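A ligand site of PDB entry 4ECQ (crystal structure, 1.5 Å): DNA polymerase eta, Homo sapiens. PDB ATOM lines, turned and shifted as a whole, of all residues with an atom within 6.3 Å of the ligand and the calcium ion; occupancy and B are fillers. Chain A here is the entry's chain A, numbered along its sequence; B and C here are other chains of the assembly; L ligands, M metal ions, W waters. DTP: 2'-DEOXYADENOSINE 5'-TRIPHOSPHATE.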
ATOM      1  N   ASP A  16      -1.400  19.162 -18.670  1.00  0.00           N
ATOM      2  CA  ASP A  16       0.032  18.951 -18.954  1.00  0.00           C
ATOM      3  C   ASP A  16       0.256  17.440 -18.926  1.00  0.00           C
ATOM      4  O   ASP A  16       0.109  16.817 -17.865  1.00  0.00           O
ATOM      5  CB  ASP A  16       0.802  19.643 -17.824  1.00  0.00           C
ATOM      6  CG  ASP A  16       2.289  19.749 -18.069  1.00  0.00           C
ATOM      7  OD1 ASP A  16       2.954  20.521 -17.332  1.00  0.00           O
ATOM      8  OD2 ASP A  16       2.802  19.074 -18.957  1.00  0.00           O
ATOM      9  N   MET A  17       0.603  16.830 -20.060  1.00  0.00           N
ATOM     10  CA  MET A  17       0.797  15.377 -20.107  1.00  0.00           C
ATOM     11  C   MET A  17       1.965  14.970 -19.217  1.00  0.00           C
ATOM     12  O   MET A  17       2.971  15.672 -19.130  1.00  0.00           O
ATOM     13  CB  MET A  17       1.052  14.911 -21.536  1.00  0.00           C
ATOM     14  CG  MET A  17       0.008  15.407 -22.544  1.00  0.00           C
ATOM     15  SD  MET A  17      -1.674  14.917 -22.113  1.00  0.00           S
ATOM     16  CE  MET A  17      -1.519  13.157 -22.168  1.00  0.00           C
ATOM     17  N   ASP A  18       1.828  13.851 -18.528  1.00  0.00           N
ATOM     18  CA  ASP A  18       2.934  13.385 -17.691  1.00  0.00           C
ATOM     19  C   ASP A  18       4.027  12.775 -18.569  1.00  0.00           C
ATOM     20  O   ASP A  18       3.733  12.037 -19.543  1.00  0.00           O
ATOM     21  CB  ASP A  18       2.440  12.347 -16.701  1.00  0.00           C
ATOM     22  CG  ASP A  18       1.395  12.913 -15.729  1.00  0.00           C
ATOM     23  OD1 ASP A  18       1.500  14.098 -15.386  1.00  0.00           O
ATOM     24  OD2 ASP A  18       0.513  12.158 -15.300  1.00  0.00           O
ATOM     25  N   CYS A  19       5.272  13.096 -18.222  1.00  0.00           N
ATOM     26  CA  CYS A  19       6.454  12.561 -18.938  1.00  0.00           C
ATOM     27  C   CYS A  19       6.134  12.178 -20.376  1.00  0.00           C
ATOM     28  O   CYS A  19       6.247  11.020 -20.764  1.00  0.00           O
ATOM     29  CB  CYS A  19       7.101  11.405 -18.171  1.00  0.00           C
ATOM     30  SG  CYS A  19       6.073  10.002 -17.710  1.00  0.00           S
ATOM     31  N   PHE A  20       5.751  13.171 -21.183  1.00  0.00           N
ATOM     32  CA  PHE A  20       5.006  12.885 -22.407  1.00  0.00           C
ATOM     33  C   PHE A  20       5.723  11.970 -23.397  1.00  0.00           C
ATOM     34  O   PHE A  20       5.142  10.972 -23.837  1.00  0.00           O
ATOM     35  CB  PHE A  20       4.591  14.188 -23.098  1.00  0.00           C
ATOM     36  CG  PHE A  20       3.735  13.976 -24.317  1.00  0.00           C
ATOM     37  CD1 PHE A  20       2.601  13.181 -24.257  1.00  0.00           C
ATOM     38  CD2 PHE A  20       4.047  14.618 -25.505  1.00  0.00           C
ATOM     39  CE1 PHE A  20       1.805  12.990 -25.394  1.00  0.00           C
ATOM     40  CE2 PHE A  20       3.236  14.427 -26.645  1.00  0.00           C
ATOM     41  CZ  PHE A  20       2.130  13.626 -26.568  1.00  0.00           C
ATOM     42  N   PHE A  21       6.962  12.285 -23.795  1.00  0.00           N
ATOM     43  CA  PHE A  21       7.592  11.455 -24.812  1.00  0.00           C
ATOM     44  C   PHE A  21       7.773  10.015 -24.305  1.00  0.00           C
ATOM     45  O   PHE A  21       7.740   9.079 -25.103  1.00  0.00           O
ATOM     46  CB  PHE A  21       8.948  12.008 -25.289  1.00  0.00           C
ATOM     47  CG  PHE A  21       8.873  13.262 -26.110  1.00  0.00           C
ATOM     48  CD1 PHE A  21       7.729  14.047 -26.159  1.00  0.00           C
ATOM     49  CD2 PHE A  21       9.975  13.663 -26.830  1.00  0.00           C
ATOM     50  CE1 PHE A  21       7.696  15.202 -26.933  1.00  0.00           C
ATOM     51  CE2 PHE A  21       9.956  14.827 -27.599  1.00  0.00           C
ATOM     52  CZ  PHE A  21       8.813  15.588 -27.644  1.00  0.00           C
ATOM     53  N   VAL A  22       8.011   9.867 -23.000  1.00  0.00           N
ATOM     54  CA  VAL A  22       8.102   8.545 -22.391  1.00  0.00           C
ATOM     55  C   VAL A  22       6.794   7.788 -22.552  1.00  0.00           C
ATOM     56  O   VAL A  22       6.803   6.612 -22.951  1.00  0.00           O
ATOM     57  CB  VAL A  22       8.520   8.639 -20.922  1.00  0.00           C
ATOM     58  CG1 VAL A  22       8.229   7.323 -20.175  1.00  0.00           C
ATOM     59  CG2 VAL A  22       9.993   9.004 -20.820  1.00  0.00           C
ATOM     60  N   GLN A  41      18.099  11.347 -27.463  1.00  0.00           N
ATOM     61  CA  GLN A  41      18.310  11.622 -28.883  1.00  0.00           C
ATOM     62  C   GLN A  41      19.770  11.394 -29.215  1.00  0.00           C
ATOM     63  O   GLN A  41      20.660  11.771 -28.452  1.00  0.00           O
ATOM     64  CB  GLN A  41      17.845  13.023 -29.276  1.00  0.00           C
ATOM     65  CG  GLN A  41      18.290  14.127 -28.357  1.00  0.00           C
ATOM     66  CD  GLN A  41      17.531  15.402 -28.620  1.00  0.00           C
ATOM     67  OE1 GLN A  41      16.552  15.415 -29.366  1.00  0.00           O
ATOM     68  NE2 GLN A  41      17.986  16.491 -28.014  1.00  0.00           N
ATOM     69  N   ILE A  51      15.908  13.546 -23.019  1.00  0.00           N
ATOM     70  CA  ILE A  51      14.928  14.616 -23.139  1.00  0.00           C
ATOM     71  C   ILE A  51      13.627  14.361 -22.376  1.00  0.00           C
ATOM     72  O   ILE A  51      12.813  15.281 -22.215  1.00  0.00           O
ATOM     73  CB  ILE A  51      14.622  14.957 -24.612  1.00  0.00           C
ATOM     74  CG1 ILE A  51      14.064  13.745 -25.375  1.00  0.00           C
ATOM     75  CG2 ILE A  51      15.888  15.514 -25.289  1.00  0.00           C
ATOM     76  CD1 ILE A  51      13.517  14.129 -26.768  1.00  0.00           C
ATOM     77  N   ALA A  52      13.412  13.143 -21.884  1.00  0.00           N
ATOM     78  CA  ALA A  52      12.214  12.854 -21.073  1.00  0.00           C
ATOM     79  C   ALA A  52      12.491  11.657 -20.185  1.00  0.00           C
ATOM     80  O   ALA A  52      13.225  10.743 -20.568  1.00  0.00           O
ATOM     81  CB  ALA A  52      11.000  12.590 -21.975  1.00  0.00           C
ATOM     82  N   VAL A  53      11.886  11.647 -18.990  1.00  0.00           N
ATOM     83  CA  VAL A  53      12.216  10.679 -17.941  1.00  0.00           C
ATOM     84  C   VAL A  53      10.973  10.193 -17.200  1.00  0.00           C
ATOM     85  O   VAL A  53      10.170  11.011 -16.738  1.00  0.00           O
ATOM     86  CB  VAL A  53      13.154  11.341 -16.891  1.00  0.00           C
ATOM     87  CG1 VAL A  53      13.675  10.294 -15.906  1.00  0.00           C
ATOM     88  CG2 VAL A  53      14.320  12.031 -17.561  1.00  0.00           C
ATOM     89  N   TYR A  55       8.650   8.639 -14.187  1.00  0.00           N
ATOM     90  CA  TYR A  55       8.690   8.944 -12.753  1.00  0.00           C
ATOM     91  C   TYR A  55       9.484   7.905 -11.957  1.00  0.00           C
ATOM     92  O   TYR A  55      10.143   8.230 -10.977  1.00  0.00           O
ATOM     93  CB  TYR A  55       7.265   9.197 -12.203  1.00  0.00           C
ATOM     94  CG  TYR A  55       6.765  10.578 -12.586  1.00  0.00           C
ATOM     95  CD1 TYR A  55       6.297  10.847 -13.872  1.00  0.00           C
ATOM     96  CD2 TYR A  55       6.859  11.647 -11.703  1.00  0.00           C
ATOM     97  CE1 TYR A  55       5.895  12.113 -14.251  1.00  0.00           C
ATOM     98  CE2 TYR A  55       6.447  12.911 -12.060  1.00  0.00           C
ATOM     99  CZ  TYR A  55       5.979  13.149 -13.330  1.00  0.00           C
ATOM    100  OH  TYR A  55       5.577  14.434 -13.659  1.00  0.00           O
ATOM    101  N   ARG A  58      13.003   9.044 -12.356  1.00  0.00           N
ATOM    102  CA  ARG A  58      13.288  10.263 -11.583  1.00  0.00           C
ATOM    103  C   ARG A  58      13.637   9.946 -10.125  1.00  0.00           C
ATOM    104  O   ARG A  58      14.440  10.672  -9.504  1.00  0.00           O
ATOM    105  CB  ARG A  58      12.111  11.233 -11.623  1.00  0.00           C
ATOM    106  CG  ARG A  58      11.774  11.690 -13.020  1.00  0.00           C
ATOM    107  CD  ARG A  58      10.581  12.630 -13.029  1.00  0.00           C
ATOM    108  NE  ARG A  58      10.066  12.751 -14.391  1.00  0.00           N
ATOM    109  CZ  ARG A  58       9.264  13.728 -14.811  1.00  0.00           C
ATOM    110  NH1 ARG A  58       8.864  14.669 -13.971  1.00  0.00           N
ATOM    111  NH2 ARG A  58       8.853  13.728 -16.091  1.00  0.00           N
ATOM    112  N   ARG A  64      16.316  15.323 -17.306  1.00  0.00           N
ATOM    113  CA  ARG A  64      16.549  15.888 -18.624  1.00  0.00           C
ATOM    114  C   ARG A  64      17.918  16.568 -18.692  1.00  0.00           C
ATOM    115  O   ARG A  64      18.414  17.091 -17.694  1.00  0.00           O
ATOM    116  CB  ARG A  64      15.426  16.886 -18.942  1.00  0.00           C
ATOM    117  CG  ARG A  64      15.604  17.705 -20.217  1.00  0.00           C
ATOM    118  CD  ARG A  64      14.324  18.507 -20.502  1.00  0.00           C
ATOM    119  NE  ARG A  64      13.180  17.618 -20.655  1.00  0.00           N
ATOM    120  CZ  ARG A  64      12.003  17.777 -20.043  1.00  0.00           C
ATOM    121  NH1 ARG A  64      11.808  18.817 -19.235  1.00  0.00           N
ATOM    122  NH2 ARG A  64      11.021  16.904 -20.252  1.00  0.00           N
ATOM    123  N   SER A 116       2.196  24.193 -25.782  1.00  0.00           N
ATOM    124  CA  SER A 116       3.409  23.471 -26.137  1.00  0.00           C
ATOM    125  C   SER A 116       2.999  22.120 -26.711  1.00  0.00           C
ATOM    126  O   SER A 116       1.811  21.838 -26.838  1.00  0.00           O
ATOM    127  CB  SER A 116       4.268  23.220 -24.902  1.00  0.00           C
ATOM    128  OG  SER A 116       3.686  22.211 -24.074  1.00  0.00           O
ATOM    129  N   ILE A 117       3.977  21.275 -27.018  1.00  0.00           N
ATOM    130  CA  ILE A 117       3.678  19.964 -27.576  1.00  0.00           C
ATOM    131  C   ILE A 117       2.760  19.127 -26.654  1.00  0.00           C
ATOM    132  O   ILE A 117       2.017  18.268 -27.115  1.00  0.00           O
ATOM    133  CB  ILE A 117       4.968  19.194 -27.909  1.00  0.00           C
ATOM    134  CG1 ILE A 117       4.656  18.065 -28.902  1.00  0.00           C
ATOM    135  CG2 ILE A 117       5.667  18.708 -26.654  1.00  0.00           C
ATOM    136  CD1 ILE A 117       5.873  17.565 -29.677  1.00  0.00           C
ATOM    137  N   ASP A 118       2.803  19.385 -25.343  1.00  0.00           N
ATOM    138  CA  ASP A 118       2.008  18.556 -24.430  1.00  0.00           C
ATOM    139  C   ASP A 118       1.214  19.306 -23.383  1.00  0.00           C
ATOM    140  O   ASP A 118       0.792  18.719 -22.369  1.00  0.00           O
ATOM    141  CB  ASP A 118       2.892  17.501 -23.778  1.00  0.00           C
ATOM    142  CG  ASP A 118       3.620  18.026 -22.580  1.00  0.00           C
ATOM    143  OD1 ASP A 118       3.801  17.250 -21.627  1.00  0.00           O
ATOM    144  OD2 ASP A 118       3.986  19.240 -22.576  1.00  0.00           O
ATOM    145  N   GLU A 119       0.984  20.602 -23.609  1.00  0.00           N
ATOM    146  CA  GLU A 119       0.230  21.429 -22.678  1.00  0.00           C
ATOM    147  C   GLU A 119      -0.794  22.241 -23.418  1.00  0.00           C
ATOM    148  O   GLU A 119      -0.517  22.779 -24.504  1.00  0.00           O
ATOM    149  CB  GLU A 119       1.148  22.427 -21.965  1.00  0.00           C
ATOM    150  CG  GLU A 119       2.191  21.791 -21.056  1.00  0.00           C
ATOM    151  CD  GLU A 119       2.913  22.803 -20.201  1.00  0.00           C
ATOM    152  OE1 GLU A 119       2.462  23.967 -20.140  1.00  0.00           O
ATOM    153  OE2 GLU A 119       3.940  22.438 -19.574  1.00  0.00           O
ATOM    154  N   LYS A 234       1.789  16.133  -9.175  1.00  0.00           N
ATOM    155  CA  LYS A 234       2.062  15.374 -10.389  1.00  0.00           C
ATOM    156  C   LYS A 234       2.665  14.073  -9.897  1.00  0.00           C
ATOM    157  O   LYS A 234       3.285  14.032  -8.836  1.00  0.00           O
ATOM    158  CB  LYS A 234       3.079  16.105 -11.261  1.00  0.00           C
ATOM    159  CG  LYS A 234       2.485  16.967 -12.384  1.00  0.00           C
ATOM    160  CD  LYS A 234       3.481  17.013 -13.579  1.00  0.00           C
ATOM    161  CE  LYS A 234       2.872  17.627 -14.861  1.00  0.00           C
ATOM    162  NZ  LYS A 234       2.557  16.614 -15.945  1.00  0.00           N
ATOM    163  N   PRO A 235       2.470  12.992 -10.651  1.00  0.00           N
ATOM    164  CA  PRO A 235       1.733  12.907 -11.911  1.00  0.00           C
ATOM    165  C   PRO A 235       0.313  12.398 -11.683  1.00  0.00           C
ATOM    166  O   PRO A 235      -0.053  11.995 -10.573  1.00  0.00           O
ATOM    167  CB  PRO A 235       2.506  11.833 -12.651  1.00  0.00           C
ATOM    168  CG  PRO A 235       2.880  10.853 -11.548  1.00  0.00           C
ATOM    169  CD  PRO A 235       3.151  11.721 -10.329  1.00  0.00           C
ATOM    170  P    DT B   3      27.500  20.383 -22.783  1.00  0.00           P
ATOM    171  OP1  DT B   3      28.618  21.309 -22.492  1.00  0.00           O
ATOM    172  OP2  DT B   3      27.057  19.408 -21.771  1.00  0.00           O
ATOM    173  O5'  DT B   3      26.240  21.271 -23.205  1.00  0.00           O
ATOM    174  C5'  DT B   3      24.923  20.740 -23.108  1.00  0.00           C
ATOM    175  C4'  DT B   3      24.613  19.816 -24.273  1.00  0.00           C
ATOM    176  O4'  DT B   3      23.439  19.024 -23.948  1.00  0.00           O
ATOM    177  C3'  DT B   3      24.282  20.506 -25.592  1.00  0.00           C
ATOM    178  O3'  DT B   3      24.678  19.667 -26.669  1.00  0.00           O
ATOM    179  C2'  DT B   3      22.766  20.645 -25.516  1.00  0.00           C
ATOM    180  C1'  DT B   3      22.384  19.333 -24.841  1.00  0.00           C
ATOM    181  N1   DT B   3      21.124  19.402 -24.036  1.00  0.00           N
ATOM    182  C2   DT B   3      20.137  18.461 -24.225  1.00  0.00           C
ATOM    183  O2   DT B   3      20.223  17.535 -25.015  1.00  0.00           O
ATOM    184  N3   DT B   3      19.030  18.626 -23.435  1.00  0.00           N
ATOM    185  C4   DT B   3      18.815  19.619 -22.501  1.00  0.00           C
ATOM    186  O4   DT B   3      17.786  19.689 -21.835  1.00  0.00           O
ATOM    187  C5   DT B   3      19.884  20.579 -22.349  1.00  0.00           C
ATOM    188  C7   DT B   3      19.777  21.710 -21.371  1.00  0.00           C
ATOM    189  C6   DT B   3      20.974  20.425 -23.120  1.00  0.00           C
ATOM    190  P    DT B   4      24.309  20.055 -28.179  1.00  0.00           P
ATOM    191  OP1  DT B   4      25.112  19.196 -29.082  1.00  0.00           O
ATOM    192  OP2  DT B   4      24.351  21.518 -28.313  1.00  0.00           O
ATOM    193  O5'  DT B   4      22.765  19.614 -28.304  1.00  0.00           O
ATOM    194  C5'  DT B   4      22.463  18.246 -28.474  1.00  0.00           C
ATOM    195  C4'  DT B   4      21.099  18.155 -29.112  1.00  0.00           C
ATOM    196  O4'  DT B   4      20.093  18.485 -28.118  1.00  0.00           O
ATOM    197  C3'  DT B   4      20.821  19.089 -30.279  1.00  0.00           C
ATOM    198  O3'  DT B   4      20.057  18.327 -31.189  1.00  0.00           O
ATOM    199  C2'  DT B   4      20.002  20.220 -29.658  1.00  0.00           C
ATOM    200  C1'  DT B   4      19.185  19.440 -28.649  1.00  0.00           C
ATOM    201  N1   DT B   4      18.710  20.191 -27.466  1.00  0.00           N
ATOM    202  C2   DT B   4      17.479  19.821 -26.984  1.00  0.00           C
ATOM    203  O2   DT B   4      16.815  18.948 -27.509  1.00  0.00           O
ATOM    204  N3   DT B   4      17.068  20.510 -25.886  1.00  0.00           N
ATOM    205  C4   DT B   4      17.749  21.501 -25.214  1.00  0.00           C
ATOM    206  O4   DT B   4      17.274  22.050 -24.230  1.00  0.00           O
ATOM    207  C5   DT B   4      19.042  21.843 -25.779  1.00  0.00           C
ATOM    208  C7   DT B   4      19.881  22.918 -25.144  1.00  0.00           C
ATOM    209  C6   DT B   4      19.458  21.168 -26.861  1.00  0.00           C
ATOM    210  P    DA B   5      19.566  18.953 -32.575  1.00  0.00           P
ATOM    211  OP1  DA B   5      19.762  17.940 -33.627  1.00  0.00           O
ATOM    212  OP2  DA B   5      20.211  20.285 -32.731  1.00  0.00           O
ATOM    213  O5'  DA B   5      18.018  19.213 -32.347  1.00  0.00           O
ATOM    214  C5'  DA B   5      17.125  18.095 -32.245  1.00  0.00           C
ATOM    215  C4'  DA B   5      15.708  18.593 -32.094  1.00  0.00           C
ATOM    216  O4'  DA B   5      15.560  19.260 -30.805  1.00  0.00           O
ATOM    217  C3'  DA B   5      15.303  19.633 -33.144  1.00  0.00           C
ATOM    218  O3'  DA B   5      13.950  19.375 -33.507  1.00  0.00           O
ATOM    219  C2'  DA B   5      15.427  20.951 -32.381  1.00  0.00           C
ATOM    220  C1'  DA B   5      14.918  20.500 -31.019  1.00  0.00           C
ATOM    221  N9   DA B   5      15.290  21.412 -29.945  1.00  0.00           N
ATOM    222  C8   DA B   5      16.455  22.113 -29.819  1.00  0.00           C
ATOM    223  N7   DA B   5      16.512  22.846 -28.717  1.00  0.00           N
ATOM    224  C5   DA B   5      15.312  22.604 -28.083  1.00  0.00           C
ATOM    225  C6   DA B   5      14.763  23.083 -26.877  1.00  0.00           C
ATOM    226  N6   DA B   5      15.384  23.946 -26.063  1.00  0.00           N
ATOM    227  N1   DA B   5      13.541  22.621 -26.540  1.00  0.00           N
ATOM    228  C2   DA B   5      12.905  21.766 -27.352  1.00  0.00           C
ATOM    229  N3   DA B   5      13.322  21.246 -28.512  1.00  0.00           N
ATOM    230  C4   DA B   5      14.538  21.722 -28.809  1.00  0.00           C
ATOM    231  P    DT C   8       6.633  26.074 -19.399  1.00  0.00           P
ATOM    232  OP1  DT C   8       5.694  27.103 -19.884  1.00  0.00           O
ATOM    233  OP2  DT C   8       6.243  25.148 -18.315  1.00  0.00           O
ATOM    234  O5'  DT C   8       7.099  25.135 -20.595  1.00  0.00           O
ATOM    235  C5'  DT C   8       6.608  23.835 -20.592  1.00  0.00           C
ATOM    236  C4'  DT C   8       6.527  23.289 -21.991  1.00  0.00           C
ATOM    237  O4'  DT C   8       7.606  23.832 -22.813  1.00  0.00           O
ATOM    238  C3'  DT C   8       6.664  21.765 -22.001  1.00  0.00           C
ATOM    239  O3'  DT C   8       5.770  21.205 -22.936  1.00  0.00           O
ATOM    240  C2'  DT C   8       8.121  21.557 -22.435  1.00  0.00           C
ATOM    241  C1'  DT C   8       8.361  22.763 -23.350  1.00  0.00           C
ATOM    242  N1   DT C   8       9.789  23.191 -23.379  1.00  0.00           N
ATOM    243  C2   DT C   8      10.564  22.825 -24.447  1.00  0.00           C
ATOM    244  O2   DT C   8      10.154  22.125 -25.370  1.00  0.00           O
ATOM    245  N3   DT C   8      11.867  23.275 -24.395  1.00  0.00           N
ATOM    246  C4   DT C   8      12.451  24.046 -23.416  1.00  0.00           C
ATOM    247  O4   DT C   8      13.621  24.408 -23.465  1.00  0.00           O
ATOM    248  C5   DT C   8      11.575  24.402 -22.332  1.00  0.00           C
ATOM    249  C7   DT C   8      12.115  25.252 -21.210  1.00  0.00           C
ATOM    250  C6   DT C   8      10.304  23.969 -22.363  1.00  0.00           C
HETATM  251  PG  DTP L   1       6.339  16.163 -16.653  1.00  0.00           P
HETATM  252  O1G DTP L   1       7.251  16.760 -15.592  1.00  0.00           O
HETATM  253  O2G DTP L   1       5.579  14.936 -16.249  1.00  0.00           O
HETATM  254  O3G DTP L   1       5.491  17.195 -17.361  1.00  0.00           O
HETATM  255  PB  DTP L   1       7.476  15.919 -19.312  1.00  0.00           P
HETATM  256  O1B DTP L   1       6.097  15.917 -19.928  1.00  0.00           O
HETATM  257  O2B DTP L   1       8.511  15.020 -19.933  1.00  0.00           O
HETATM  258  O3B DTP L   1       7.426  15.593 -17.736  1.00  0.00           O
HETATM  259  PA  DTP L   1       7.629  18.734 -20.086  1.00  0.00           P
HETATM  260  O1A DTP L   1       8.623  19.804 -19.665  1.00  0.00           O
HETATM  261  O2A DTP L   1       6.172  18.987 -19.846  1.00  0.00           O
HETATM  262  O3A DTP L   1       8.117  17.381 -19.327  1.00  0.00           O
HETATM  263  O5' DTP L   1       7.916  18.475 -21.641  1.00  0.00           O
HETATM  264  C5' DTP L   1       7.015  17.779 -22.513  1.00  0.00           C
HETATM  265  C4' DTP L   1       7.851  17.062 -23.570  1.00  0.00           C
HETATM  266  O4' DTP L   1       8.598  18.020 -24.329  1.00  0.00           O
HETATM  267  C3' DTP L   1       8.896  16.137 -22.954  1.00  0.00           C
HETATM  268  O3' DTP L   1       8.397  14.822 -22.711  1.00  0.00           O
HETATM  269  C2' DTP L   1       9.990  16.156 -24.009  1.00  0.00           C
HETATM  270  C1' DTP L   1       9.916  17.558 -24.615  1.00  0.00           C
HETATM  271  N9  DTP L   1      10.868  18.510 -23.979  1.00  0.00           N
HETATM  272  C8  DTP L   1      10.682  19.219 -22.865  1.00  0.00           C
HETATM  273  N7  DTP L   1      11.788  19.981 -22.632  1.00  0.00           N
HETATM  274  C5  DTP L   1      12.662  19.727 -23.629  1.00  0.00           C
HETATM  275  C6  DTP L   1      13.932  20.198 -23.949  1.00  0.00           C
HETATM  276  N6  DTP L   1      14.559  21.104 -23.151  1.00  0.00           N
HETATM  277  N1  DTP L   1      14.559  19.730 -25.052  1.00  0.00           N
HETATM  278  C2  DTP L   1      13.952  18.837 -25.849  1.00  0.00           C
HETATM  279  N3  DTP L   1      12.725  18.365 -25.582  1.00  0.00           N
HETATM  280  C4  DTP L   1      12.070  18.807 -24.479  1.00  0.00           C
HETATM  281 CA    CA M   1       4.410  17.424 -19.380  1.00  0.00          CA
HETATM  282  O   HOH W   1      11.774  17.555 -28.124  1.00  0.00           O
HETATM  283  O   HOH W   2      15.240  22.132 -19.920  1.00  0.00           O
HETATM  284  O   HOH W   3       5.577  20.812 -17.838  1.00  0.00           O
HETATM  285  O   HOH W   4       8.949  20.141 -26.264  1.00  0.00           O
HETATM  286  O   HOH W   5      10.575  14.065 -18.488  1.00  0.00           O
HETATM  287  O   HOH W   6      12.666  21.677 -20.643  1.00  0.00           O
HETATM  288  O   HOH W   7       6.625  19.517 -15.357  1.00  0.00           O
HETATM  289  O   HOH W   8       9.791  17.647 -15.760  1.00  0.00           O
HETATM  290  O   HOH W   9      10.249  22.024 -19.790  1.00  0.00           O
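Lys 234 touches the calcium ion (NZ to CA, 3.99 Å).
Within 4 Å of the calcium ion: Asp 16, Met 17, Asp 118 and Lys 234.
A nitrogen (N1) of the ligand sits close to N1 of DA 5 of chain B (3.4 Å).
Asp 18 touches the ligand (CA to O2G, 3.4 Å).
Ile 51 touches the ligand (O to C2', 3.5 Å).
Ala 52 touches the ligand (CB to O3', 3.5 Å).
Ile 117 touches the ligand (CG2 to O4', 3.8 Å).
DT 3 of chain B touches the ligand (O4 to N6, 3.8 Å).
Hydrophobic or aromatic side chains within 4 Å of the ligand: Phe 20, Phe 21, Ile 51, Ala 52, Tyr 55 and Ile 117.
Of the 24 residues printed, 18 come within 4 Å of the ligand.
Along chain A the residues within 4 Å of the ligand span positions 16 to 234.
The backbone carbonyl oxygen (O) of Met 17 binds the calcium ion, at 2.3 Å.
An oxygen (O3G) of the ligand is bound to the calcium ion, 2.3 Å away.
O1B of the ligand binds the calcium ion, 2.3 Å away.
The calcium ion is bound by OD1 of Asp 118 (2.3 Å).
The side-chain carboxylate (OD2) of Asp 16 is bound to the calcium ion.
The calcium ion is bound by O2A of the ligand.
Water W6 lies within hydrogen-bond range of a nitrogen (N7) of the ligand (2.8 Å) and the guanidinium group (NH1) of Arg 64 (3.3 Å).
Water W3 bridges OD1 of Asp 16 (2.7 Å) and OE2 of Glu 119 (2.9 Å).
Water W4 bridges O2 of DT 8 of chain C (2.5 Å) and an oxygen (O4') of the ligand (2.9 Å).
O2G of the ligand lies within hydrogen-bond range of OH of Tyr 55 (2.6 Å).
O3' of the ligand sits at hydrogen-bond distance from N of Phe 20, 3.5 Å away.
An oxygen (O2B) of the ligand is in salt-bridge range of the guanidinium group (NH2) of Arg 64.
A nitrogen (N6) of the ligand sits at hydrogen-bond distance from O4 of DT 4 of chain B (3.1 Å).
The backbone NH of Cys 19 lies within hydrogen-bond range of an oxygen (O2G) of the ligand, at 2.7 Å.
An oxygen (O1G) of the ligand is in salt-bridge range of the guanidinium group (NH1) of Arg 58.
An oxygen (O2G) of the ligand is in salt-bridge range of the side-chain amino group (NZ) of Lys 234 (3.5 Å).
N of Phe 21 sits at hydrogen-bond distance from O3' of the ligand (3.1 Å).
O4 of DT 8 of chain C sits at hydrogen-bond distance from a nitrogen (N6) of the ligand.
N of Asp 118 sits close to OG of Ser 116 (3.2 Å).
O of Met 17 lies close to NZ of Lys 234.
NH1 of Arg 58 sits at hydrogen-bond distance from OH of Tyr 55 (3.3 Å).
OD2 of Asp 118 lies close to O3' of DT 8 of chain C (2.7 Å).
NZ of Lys 234 sits at hydrogen-bond distance from O of Asp 16.
O2 of DT 4 of chain B is in hydrogen-bond range of NE2 of Gln 41, 2.8 Å away.
The guanidinium group of Arg 58 sits at hydrogen-bond distance from the backbone carbonyl oxygen of Val 53 (2.9 Å).
The side-chain amino group of Lys 234 is in salt-bridge range of the side-chain carboxylate of Asp 18.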
